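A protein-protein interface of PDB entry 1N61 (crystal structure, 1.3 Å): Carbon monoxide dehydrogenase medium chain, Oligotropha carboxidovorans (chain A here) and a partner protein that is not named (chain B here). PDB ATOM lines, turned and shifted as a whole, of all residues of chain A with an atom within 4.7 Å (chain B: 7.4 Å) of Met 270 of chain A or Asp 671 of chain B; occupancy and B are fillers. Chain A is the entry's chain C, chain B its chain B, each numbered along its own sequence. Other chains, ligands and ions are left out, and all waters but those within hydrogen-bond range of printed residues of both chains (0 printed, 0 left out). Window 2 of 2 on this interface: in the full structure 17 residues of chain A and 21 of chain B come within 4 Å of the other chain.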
ATOM      1  N   LEU A 186       1.342  21.365  11.452  1.00  0.00           N
ATOM      2  CA  LEU A 186       2.106  20.875  12.581  1.00  0.00           C
ATOM      3  C   LEU A 186       1.453  19.623  13.087  1.00  0.00           C
ATOM      4  O   LEU A 186       0.269  19.649  13.358  1.00  0.00           O
ATOM      5  CB  LEU A 186       2.121  21.919  13.703  1.00  0.00           C
ATOM      6  CG  LEU A 186       2.931  21.536  14.925  1.00  0.00           C
ATOM      7  CD1 LEU A 186       4.363  21.233  14.585  1.00  0.00           C
ATOM      8  CD2 LEU A 186       2.872  22.591  15.969  1.00  0.00           C
ATOM      9  N   THR A 195      -1.971  19.328  15.041  1.00  0.00           N
ATOM     10  CA  THR A 195      -1.945  20.198  16.203  1.00  0.00           C
ATOM     11  C   THR A 195      -2.525  21.549  15.845  1.00  0.00           C
ATOM     12  O   THR A 195      -3.356  22.104  16.592  1.00  0.00           O
ATOM     13  CB  THR A 195      -0.505  20.271  16.681  1.00  0.00           C
ATOM     14  OG1 THR A 195      -0.034  18.927  16.988  1.00  0.00           O
ATOM     15  CG2 THR A 195      -0.339  21.172  17.887  1.00  0.00           C
ATOM     16  N   ALA A 196      -2.110  22.048  14.674  1.00  0.00           N
ATOM     17  CA  ALA A 196      -2.687  23.240  14.031  1.00  0.00           C
ATOM     18  C   ALA A 196      -2.204  23.223  12.619  1.00  0.00           C
ATOM     19  O   ALA A 196      -1.118  22.714  12.352  1.00  0.00           O
ATOM     20  CB  ALA A 196      -2.243  24.487  14.733  1.00  0.00           C
ATOM     21  N   TYR A 266      -1.381  26.117  23.702  1.00  0.00           N
ATOM     22  CA  TYR A 266      -0.323  25.748  22.776  1.00  0.00           C
ATOM     23  C   TYR A 266      -0.846  25.705  21.349  1.00  0.00           C
ATOM     24  O   TYR A 266      -0.247  26.242  20.414  1.00  0.00           O
ATOM     25  CB  TYR A 266       0.341  24.415  23.165  1.00  0.00           C
ATOM     26  CG  TYR A 266       1.271  23.884  22.098  1.00  0.00           C
ATOM     27  CD1 TYR A 266       2.441  24.534  21.796  1.00  0.00           C
ATOM     28  CD2 TYR A 266       1.040  22.662  21.499  1.00  0.00           C
ATOM     29  CE1 TYR A 266       3.361  23.994  20.866  1.00  0.00           C
ATOM     30  CE2 TYR A 266       1.950  22.121  20.605  1.00  0.00           C
ATOM     31  CZ  TYR A 266       3.116  22.780  20.323  1.00  0.00           C
ATOM     32  OH  TYR A 266       3.991  22.273  19.380  1.00  0.00           O
ATOM     33  N   ARG A 267      -1.978  25.067  21.177  1.00  0.00           N
ATOM     34  CA  ARG A 267      -2.554  24.928  19.838  1.00  0.00           C
ATOM     35  C   ARG A 267      -3.000  26.246  19.251  1.00  0.00           C
ATOM     36  O   ARG A 267      -2.807  26.453  18.083  1.00  0.00           O
ATOM     37  CB  ARG A 267      -3.682  23.934  19.874  1.00  0.00           C
ATOM     38  CG  ARG A 267      -3.109  22.557  20.280  1.00  0.00           C
ATOM     39  CD  ARG A 267      -4.088  21.483  20.352  1.00  0.00           C
ATOM     40  NE  ARG A 267      -4.539  21.107  19.016  1.00  0.00           N
ATOM     41  CZ  ARG A 267      -5.344  20.100  18.800  1.00  0.00           C
ATOM     42  NH1 ARG A 267      -5.972  19.576  19.816  1.00  0.00           N
ATOM     43  NH2 ARG A 267      -5.644  19.721  17.563  1.00  0.00           N
ATOM     44  N   THR A 268      -3.475  27.162  20.082  1.00  0.00           N
ATOM     45  CA  THR A 268      -3.778  28.503  19.589  1.00  0.00           C
ATOM     46  C   THR A 268      -2.495  29.163  19.104  1.00  0.00           C
ATOM     47  O   THR A 268      -2.455  29.760  18.021  1.00  0.00           O
ATOM     48  CB  THR A 268      -4.454  29.335  20.717  1.00  0.00           C
ATOM     49  OG1 THR A 268      -5.788  28.833  20.930  1.00  0.00           O
ATOM     50  CG2 THR A 268      -4.617  30.824  20.367  1.00  0.00           C
ATOM     51  N   LYS A 269      -1.437  29.087  19.903  1.00  0.00           N
ATOM     52  CA  LYS A 269      -0.191  29.709  19.489  1.00  0.00           C
ATOM     53  C   LYS A 269       0.321  29.076  18.215  1.00  0.00           C
ATOM     54  O   LYS A 269       0.939  29.751  17.395  1.00  0.00           O
ATOM     55  CB  LYS A 269       0.831  29.714  20.621  1.00  0.00           C
ATOM     56  CG  LYS A 269       0.411  30.552  21.820  1.00  0.00           C
ATOM     57  CD  LYS A 269       0.287  32.044  21.425  1.00  0.00           C
ATOM     58  CE  LYS A 269      -0.137  33.005  22.515  1.00  0.00           C
ATOM     59  NZ  LYS A 269      -0.116  34.307  21.814  1.00  0.00           N
ATOM     60  N   MET A 270       0.210  27.759  18.100  1.00  0.00           N
ATOM     61  CA  MET A 270       0.669  27.099  16.912  1.00  0.00           C
ATOM     62  C   MET A 270      -0.124  27.491  15.671  1.00  0.00           C
ATOM     63  O   MET A 270       0.406  27.451  14.571  1.00  0.00           O
ATOM     64  CB  MET A 270       0.698  25.573  17.103  1.00  0.00           C
ATOM     65  CG  MET A 270       1.752  25.114  18.078  1.00  0.00           C
ATOM     66  SD  MET A 270       3.445  25.730  17.817  1.00  0.00           S
ATOM     67  CE  MET A 270       3.542  27.184  18.929  1.00  0.00           C
ATOM     68  N   ALA A 271      -1.410  27.763  15.826  1.00  0.00           N
ATOM     69  CA  ALA A 271      -2.165  28.297  14.694  1.00  0.00           C
ATOM     70  C   ALA A 271      -1.491  29.570  14.182  1.00  0.00           C
ATOM     71  O   ALA A 271      -1.384  29.801  12.993  1.00  0.00           O
ATOM     72  CB  ALA A 271      -3.595  28.600  15.118  1.00  0.00           C
ATOM     73  N   GLY A 272      -1.058  30.425  15.102  1.00  0.00           N
ATOM     74  CA  GLY A 272      -0.405  31.675  14.705  1.00  0.00           C
ATOM     75  C   GLY A 272       0.951  31.418  14.055  1.00  0.00           C
ATOM     76  O   GLY A 272       1.293  32.044  13.050  1.00  0.00           O
ATOM     77  N   VAL A 273       1.727  30.467  14.601  1.00  0.00           N
ATOM     78  CA  VAL A 273       2.973  30.148  13.934  1.00  0.00           C
ATOM     79  C   VAL A 273       2.764  29.536  12.553  1.00  0.00           C
ATOM     80  O   VAL A 273       3.495  29.886  11.598  1.00  0.00           O
ATOM     81  CB  VAL A 273       3.846  29.213  14.826  1.00  0.00           C
ATOM     82  CG1 VAL A 273       5.143  28.837  14.105  1.00  0.00           C
ATOM     83  CG2 VAL A 273       4.134  29.855  16.154  1.00  0.00           C
ATOM     84  N   MET A 274       1.824  28.601  12.434  1.00  0.00           N
ATOM     85  CA  MET A 274       1.542  28.047  11.133  1.00  0.00           C
ATOM     86  C   MET A 274       1.094  29.116  10.147  1.00  0.00           C
ATOM     87  O   MET A 274       1.459  29.088   8.975  1.00  0.00           O
ATOM     88  CB  MET A 274       0.538  26.919  11.247  1.00  0.00           C
ATOM     89  CG  MET A 274       1.062  25.683  12.011  1.00  0.00           C
ATOM     90  SD  MET A 274       2.540  24.933  11.332  1.00  0.00           S
ATOM     91  CE  MET A 274       3.689  25.436  12.444  1.00  0.00           C
ATOM     92  N   PHE B 470      21.778  32.899  19.267  1.00  0.00           N
ATOM     93  CA  PHE B 470      20.454  32.927  19.874  1.00  0.00           C
ATOM     94  C   PHE B 470      20.307  34.177  20.715  1.00  0.00           C
ATOM     95  O   PHE B 470      19.305  34.900  20.590  1.00  0.00           O
ATOM     96  CB  PHE B 470      20.241  31.670  20.746  1.00  0.00           C
ATOM     97  CG  PHE B 470      18.872  31.581  21.362  1.00  0.00           C
ATOM     98  CD1 PHE B 470      17.842  30.946  20.704  1.00  0.00           C
ATOM     99  CD2 PHE B 470      18.615  32.155  22.589  1.00  0.00           C
ATOM    100  CE1 PHE B 470      16.629  30.851  21.271  1.00  0.00           C
ATOM    101  CE2 PHE B 470      17.353  32.088  23.135  1.00  0.00           C
ATOM    102  CZ  PHE B 470      16.355  31.475  22.457  1.00  0.00           C
ATOM    103  N   THR B 475      18.674  33.519  15.610  1.00  0.00           N
ATOM    104  CA  THR B 475      18.119  32.191  15.402  1.00  0.00           C
ATOM    105  C   THR B 475      17.149  31.864  16.525  1.00  0.00           C
ATOM    106  O   THR B 475      17.347  32.297  17.649  1.00  0.00           O
ATOM    107  CB  THR B 475      19.243  31.113  15.324  1.00  0.00           C
ATOM    108  OG1 THR B 475      18.672  29.821  15.031  1.00  0.00           O
ATOM    109  CG2 THR B 475      19.898  30.974  16.665  1.00  0.00           C
ATOM    110  N   ARG B 476      16.210  30.980  16.241  1.00  0.00           N
ATOM    111  CA  ARG B 476      15.306  30.455  17.256  1.00  0.00           C
ATOM    112  C   ARG B 476      15.529  28.956  17.398  1.00  0.00           C
ATOM    113  O   ARG B 476      14.798  28.317  18.115  1.00  0.00           O
ATOM    114  CB  ARG B 476      13.883  30.690  16.803  1.00  0.00           C
ATOM    115  CG  ARG B 476      13.558  32.197  16.594  1.00  0.00           C
ATOM    116  CD  ARG B 476      13.770  33.044  17.852  1.00  0.00           C
ATOM    117  NE  ARG B 476      12.861  32.601  18.897  1.00  0.00           N
ATOM    118  CZ  ARG B 476      12.917  32.976  20.169  1.00  0.00           C
ATOM    119  NH1 ARG B 476      13.941  33.652  20.665  1.00  0.00           N
ATOM    120  NH2 ARG B 476      11.913  32.691  20.948  1.00  0.00           N
ATOM    121  N   GLU B 477      16.667  28.471  16.919  1.00  0.00           N
ATOM    122  CA  GLU B 477      17.047  27.077  17.071  1.00  0.00           C
ATOM    123  C   GLU B 477      18.223  26.907  18.023  1.00  0.00           C
ATOM    124  O   GLU B 477      19.076  27.775  18.117  1.00  0.00           O
ATOM    125  CB  GLU B 477      17.462  26.504  15.708  1.00  0.00           C
ATOM    126  CG  GLU B 477      18.058  25.101  15.608  1.00  0.00           C
ATOM    127  CD  GLU B 477      18.359  24.708  14.156  1.00  0.00           C
ATOM    128  OE1 GLU B 477      17.375  24.523  13.420  1.00  0.00           O
ATOM    129  OE2 GLU B 477      19.541  24.768  13.692  1.00  0.00           O
ATOM    130  N   ILE B 668      16.634  22.102  18.109  1.00  0.00           N
ATOM    131  CA  ILE B 668      15.274  22.333  18.602  1.00  0.00           C
ATOM    132  C   ILE B 668      14.813  23.755  18.264  1.00  0.00           C
ATOM    133  O   ILE B 668      15.532  24.740  18.504  1.00  0.00           O
ATOM    134  CB  ILE B 668      15.197  22.108  20.111  1.00  0.00           C
ATOM    135  CG1 ILE B 668      15.855  20.761  20.461  1.00  0.00           C
ATOM    136  CG2 ILE B 668      13.753  22.216  20.574  1.00  0.00           C
ATOM    137  CD1 ILE B 668      15.878  20.473  21.955  1.00  0.00           C
ATOM    138  N   ASP B 669      13.610  23.871  17.731  1.00  0.00           N
ATOM    139  CA  ASP B 669      12.946  25.151  17.503  1.00  0.00           C
ATOM    140  C   ASP B 669      12.213  25.543  18.751  1.00  0.00           C
ATOM    141  O   ASP B 669      11.264  24.857  19.126  1.00  0.00           O
ATOM    142  CB  ASP B 669      11.968  24.963  16.334  1.00  0.00           C
ATOM    143  CG  ASP B 669      11.188  26.180  15.973  1.00  0.00           C
ATOM    144  OD1 ASP B 669      10.890  27.065  16.815  1.00  0.00           O
ATOM    145  OD2 ASP B 669      10.849  26.301  14.778  1.00  0.00           O
ATOM    146  N   VAL B 670      12.702  26.576  19.458  1.00  0.00           N
ATOM    147  CA  VAL B 670      12.105  26.924  20.741  1.00  0.00           C
ATOM    148  C   VAL B 670      10.705  27.470  20.657  1.00  0.00           C
ATOM    149  O   VAL B 670       9.982  27.451  21.650  1.00  0.00           O
ATOM    150  CB  VAL B 670      13.005  27.856  21.569  1.00  0.00           C
ATOM    151  CG1 VAL B 670      14.378  27.246  21.689  1.00  0.00           C
ATOM    152  CG2 VAL B 670      13.052  29.264  20.949  1.00  0.00           C
ATOM    153  N   ASP B 671      10.290  27.908  19.478  1.00  0.00           N
ATOM    154  CA  ASP B 671       8.990  28.514  19.289  1.00  0.00           C
ATOM    155  C   ASP B 671       7.904  27.500  19.041  1.00  0.00           C
ATOM    156  O   ASP B 671       6.781  27.773  19.415  1.00  0.00           O
ATOM    157  CB  ASP B 671       9.047  29.545  18.170  1.00  0.00           C
ATOM    158  CG  ASP B 671       9.815  30.789  18.589  1.00  0.00           C
ATOM    159  OD1 ASP B 671       9.872  31.095  19.824  1.00  0.00           O
ATOM    160  OD2 ASP B 671      10.500  31.438  17.769  1.00  0.00           O
ATOM    161  N   THR B 672       8.221  26.329  18.467  1.00  0.00           N
ATOM    162  CA  THR B 672       7.199  25.273  18.290  1.00  0.00           C
ATOM    163  C   THR B 672       7.450  24.086  19.231  1.00  0.00           C
ATOM    164  O   THR B 672       6.553  23.266  19.408  1.00  0.00           O
ATOM    165  CB  THR B 672       7.185  24.748  16.883  1.00  0.00           C
ATOM    166  OG1 THR B 672       8.487  24.250  16.589  1.00  0.00           O
ATOM    167  CG2 THR B 672       6.892  25.849  15.876  1.00  0.00           C
ATOM    168  N   GLY B 673       8.680  23.958  19.761  1.00  0.00           N
ATOM    169  CA  GLY B 673       9.110  22.802  20.522  1.00  0.00           C
ATOM    170  C   GLY B 673       9.555  21.636  19.687  1.00  0.00           C
ATOM    171  O   GLY B 673       9.846  20.565  20.235  1.00  0.00           O
ATOM    172  N   VAL B 674       9.546  21.796  18.366  1.00  0.00           N
ATOM    173  CA  VAL B 674       9.914  20.696  17.474  1.00  0.00           C
ATOM    174  C   VAL B 674      11.428  20.466  17.512  1.00  0.00           C
ATOM    175  O   VAL B 674      12.210  21.333  17.162  1.00  0.00           O
ATOM    176  CB  VAL B 674       9.429  20.944  16.042  1.00  0.00           C
ATOM    177  CG1 VAL B 674       9.924  19.845  15.084  1.00  0.00           C
ATOM    178  CG2 VAL B 674       7.883  20.958  16.011  1.00  0.00           C
ATOM    179  N   TYR B 781      18.931  23.029  26.259  1.00  0.00           N
ATOM    180  CA  TYR B 781      18.335  24.084  27.071  1.00  0.00           C
ATOM    181  C   TYR B 781      19.198  24.456  28.266  1.00  0.00           C
ATOM    182  O   TYR B 781      18.842  25.391  28.994  1.00  0.00           O
ATOM    183  CB  TYR B 781      16.970  23.660  27.588  1.00  0.00           C
ATOM    184  CG  TYR B 781      15.869  23.725  26.533  1.00  0.00           C
ATOM    185  CD1 TYR B 781      15.188  24.905  26.296  1.00  0.00           C
ATOM    186  CD2 TYR B 781      15.522  22.635  25.781  1.00  0.00           C
ATOM    187  CE1 TYR B 781      14.140  24.988  25.378  1.00  0.00           C
ATOM    188  CE2 TYR B 781      14.476  22.699  24.903  1.00  0.00           C
ATOM    189  CZ  TYR B 781      13.839  23.888  24.636  1.00  0.00           C
ATOM    190  OH  TYR B 781      12.802  23.880  23.708  1.00  0.00           O
ATOM    191  N   ALA B 795       6.620  18.044  21.183  1.00  0.00           N
ATOM    192  CA  ALA B 795       6.672  19.471  20.905  1.00  0.00           C
ATOM    193  C   ALA B 795       5.926  20.334  21.903  1.00  0.00           C
ATOM    194  O   ALA B 795       6.437  21.388  22.297  1.00  0.00           O
ATOM    195  CB  ALA B 795       6.176  19.743  19.504  1.00  0.00           C
ATOM    196  N   TRP B 796       4.723  19.919  22.342  1.00  0.00           N
ATOM    197  CA  TRP B 796       4.038  20.767  23.313  1.00  0.00           C
ATOM    198  C   TRP B 796       4.829  20.888  24.600  1.00  0.00           C
ATOM    199  O   TRP B 796       4.866  21.947  25.195  1.00  0.00           O
ATOM    200  CB  TRP B 796       2.572  20.345  23.586  1.00  0.00           C
ATOM    201  CG  TRP B 796       2.364  19.152  24.473  1.00  0.00           C
ATOM    202  CD1 TRP B 796       2.075  17.893  24.093  1.00  0.00           C
ATOM    203  CD2 TRP B 796       2.224  19.185  25.903  1.00  0.00           C
ATOM    204  NE1 TRP B 796       1.811  17.117  25.198  1.00  0.00           N
ATOM    205  CE2 TRP B 796       1.920  17.887  26.324  1.00  0.00           C
ATOM    206  CE3 TRP B 796       2.403  20.177  26.873  1.00  0.00           C
ATOM    207  CZ2 TRP B 796       1.746  17.560  27.678  1.00  0.00           C
ATOM    208  CZ3 TRP B 796       2.192  19.864  28.215  1.00  0.00           C
ATOM    209  CH2 TRP B 796       1.905  18.557  28.597  1.00  0.00           C
ATOM    210  N   LEU B 798       8.173  20.691  24.972  1.00  0.00           N
ATOM    211  CA  LEU B 798       9.340  21.567  24.819  1.00  0.00           C
ATOM    212  C   LEU B 798       8.892  23.026  24.620  1.00  0.00           C
ATOM    213  O   LEU B 798       9.552  23.948  25.089  1.00  0.00           O
ATOM    214  CB  LEU B 798      10.274  21.078  23.724  1.00  0.00           C
ATOM    215  CG  LEU B 798      10.888  19.690  23.984  1.00  0.00           C
ATOM    216  CD1 LEU B 798      11.921  19.408  22.897  1.00  0.00           C
ATOM    217  CD2 LEU B 798      11.452  19.598  25.378  1.00  0.00           C
ATOM    218  N   TRP B 799       7.733  23.212  24.004  1.00  0.00           N
ATOM    219  CA  TRP B 799       7.124  24.537  23.946  1.00  0.00           C
ATOM    220  C   TRP B 799       6.908  25.100  25.343  1.00  0.00           C
ATOM    221  O   TRP B 799       7.268  26.247  25.642  1.00  0.00           O
ATOM    222  CB  TRP B 799       5.866  24.536  23.094  1.00  0.00           C
ATOM    223  CG  TRP B 799       5.140  25.855  23.194  1.00  0.00           C
ATOM    224  CD1 TRP B 799       5.237  26.901  22.344  1.00  0.00           C
ATOM    225  CD2 TRP B 799       4.127  26.220  24.155  1.00  0.00           C
ATOM    226  NE1 TRP B 799       4.423  27.924  22.751  1.00  0.00           N
ATOM    227  CE2 TRP B 799       3.677  27.500  23.820  1.00  0.00           C
ATOM    228  CE3 TRP B 799       3.499  25.557  25.207  1.00  0.00           C
ATOM    229  CZ2 TRP B 799       2.739  28.193  24.596  1.00  0.00           C
ATOM    230  CZ3 TRP B 799       2.508  26.188  25.918  1.00  0.00           C
ATOM    231  CH2 TRP B 799       2.154  27.505  25.626  1.00  0.00           C
ATOM    232  N   GLY B 802      10.019  26.353  27.067  1.00  0.00           N
ATOM    233  CA  GLY B 802      10.334  27.701  26.631  1.00  0.00           C
ATOM    234  C   GLY B 802       9.390  28.759  27.182  1.00  0.00           C
ATOM    235  O   GLY B 802       9.796  29.885  27.438  1.00  0.00           O
ATOM    236  N   LEU B 807      10.755  32.615  26.810  1.00  0.00           N
ATOM    237  CA  LEU B 807      11.268  32.710  25.458  1.00  0.00           C
ATOM    238  C   LEU B 807      10.248  33.216  24.440  1.00  0.00           C
ATOM    239  O   LEU B 807      10.627  33.514  23.339  1.00  0.00           O
ATOM    240  CB  LEU B 807      11.749  31.351  24.987  1.00  0.00           C
ATOM    241  CG  LEU B 807      12.860  30.702  25.822  1.00  0.00           C
ATOM    242  CD1 LEU B 807      13.395  29.435  25.162  1.00  0.00           C
ATOM    243  CD2 LEU B 807      14.037  31.646  26.084  1.00  0.00           C
ATOM    244  N   HIS B 808       8.962  33.193  24.760  1.00  0.00           N
ATOM    245  CA  HIS B 808       7.936  33.519  23.761  1.00  0.00           C
ATOM    246  C   HIS B 808       7.363  34.925  23.956  1.00  0.00           C
ATOM    247  O   HIS B 808       6.383  35.289  23.294  1.00  0.00           O
ATOM    248  CB  HIS B 808       6.790  32.507  23.740  1.00  0.00           C
ATOM    249  CG  HIS B 808       7.224  31.071  23.642  1.00  0.00           C
ATOM    250  ND1 HIS B 808       8.222  30.615  22.801  1.00  0.00           N
ATOM    251  CD2 HIS B 808       6.733  29.974  24.255  1.00  0.00           C
ATOM    252  CE1 HIS B 808       8.303  29.292  22.892  1.00  0.00           C
ATOM    253  NE2 HIS B 808       7.463  28.894  23.833  1.00  0.00           N
ATOM    254  N   VAL B 809       7.902  35.673  24.912  1.00  0.00           N
ATOM    255  CA  VAL B 809       7.352  36.985  25.254  1.00  0.00           C
ATOM    256  C   VAL B 809       7.663  37.979  24.161  1.00  0.00           C
ATOM    257  O   VAL B 809       8.791  37.982  23.656  1.00  0.00           O
ATOM    258  CB  VAL B 809       8.020  37.529  26.511  1.00  0.00           C
ATOM    259  CG1 VAL B 809       7.543  36.772  27.757  1.00  0.00           C
ATOM    260  CG2 VAL B 809       9.508  37.467  26.356  1.00  0.00           C
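The backbone carbonyl oxygen of Thr 672 of chain B sits at hydrogen-bond distance from the side-chain hydroxyl of Tyr 266 of chain A, 2.7 Å away.
The backbone NH (N) of Val 674 of chain B is in hydrogen-bond range of the side-chain hydroxyl (OG1) of Thr 672 of chain B.
The backbone carbonyl oxygen (O) of Trp 799 of chain B lies within hydrogen-bond range of a ring nitrogen (NE2) of His 808 of chain B (3.2 Å).
O of Leu 186 of chain A lies within hydrogen-bond range of N of Thr 195 of chain A (2.8 Å).
The backbone carbonyl oxygen of Val 674 of chain B lies within hydrogen-bond range of the backbone NH of Asp 669 of chain B (3.0 Å).
The backbone NH (N) of Leu 186 of chain A is in hydrogen-bond range of the side-chain sulfur (SD) of Met 274 of chain A (3.8 Å).
The guanidinium group of Arg 476 of chain B is in salt-bridge range of the side-chain carboxylate of Asp 671 of chain B, 2.8 Å away.
CG2 of Val 674 of chain B touches CD1 of Leu 186 of chain A, 3.8 Å away.
Tyr 266 of chain A touches Ala 795 of chain B (OH to CB, 3.3 Å).
Tyr 266 of chain A touches Trp 796 of chain B.
Tyr 266 of chain A touches Trp 799 of chain B (CD1 to CG, 3.3 Å).
CE of Met 270 of chain A touches O of Asp 671 of chain B, at 3.3 Å.
Met 270 of chain A touches Thr 672 of chain B.
CD1 of Trp 799 of chain B touches CE of Met 270 of chain A, at 3.8 Å.
CG1 of Val 273 of chain A touches CG2 of Thr 672 of chain B (3.9 Å).
Of chain B, only Asp 671 (3.3 Å), Thr 672 (3.8 Å) and Trp 799 (3.8 Å) come within 4 Å of Met 270 of chain A.
Asp 671 of chain B touches one residue of chain A.
Of the printed residues of chain B, Leu 186 of chain A touches Val 674.
Printed residues of chain A within 4 Å of Trp 799 of chain B: Tyr 266 and Met 270.
Printed residues of chain B within 4 Å of Tyr 266 of chain A: Thr 672 (2.7 Å), Ala 795 (3.3 Å), Trp 796 (3.5 Å) and Trp 799 (3.3 Å).
The nearest residue of chain B that does not touch Met 270 of chain A is Gly 673 of chain B (5.9 Å).
The nearest printed residue of chain B that does not touch Tyr 266 of chain A is Gly 673 of chain B (5.0 Å).
Hydrophobic or aromatic side chains of chain A that line the printed part of chain B: Leu 186, Tyr 266, Met 270 and Val 273.
Hydrophobic or aromatic side chains of chain B within 4 Å of the printed part of chain A: Val 674, Ala 795, Trp 796 and Trp 799.
Among the printed residues, 9 pairs touch across the chains.
Among the printed residues, no Asp or Glu carboxylate lies within 4 Å of a Lys or Arg side-chain nitrogen of the other chain.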
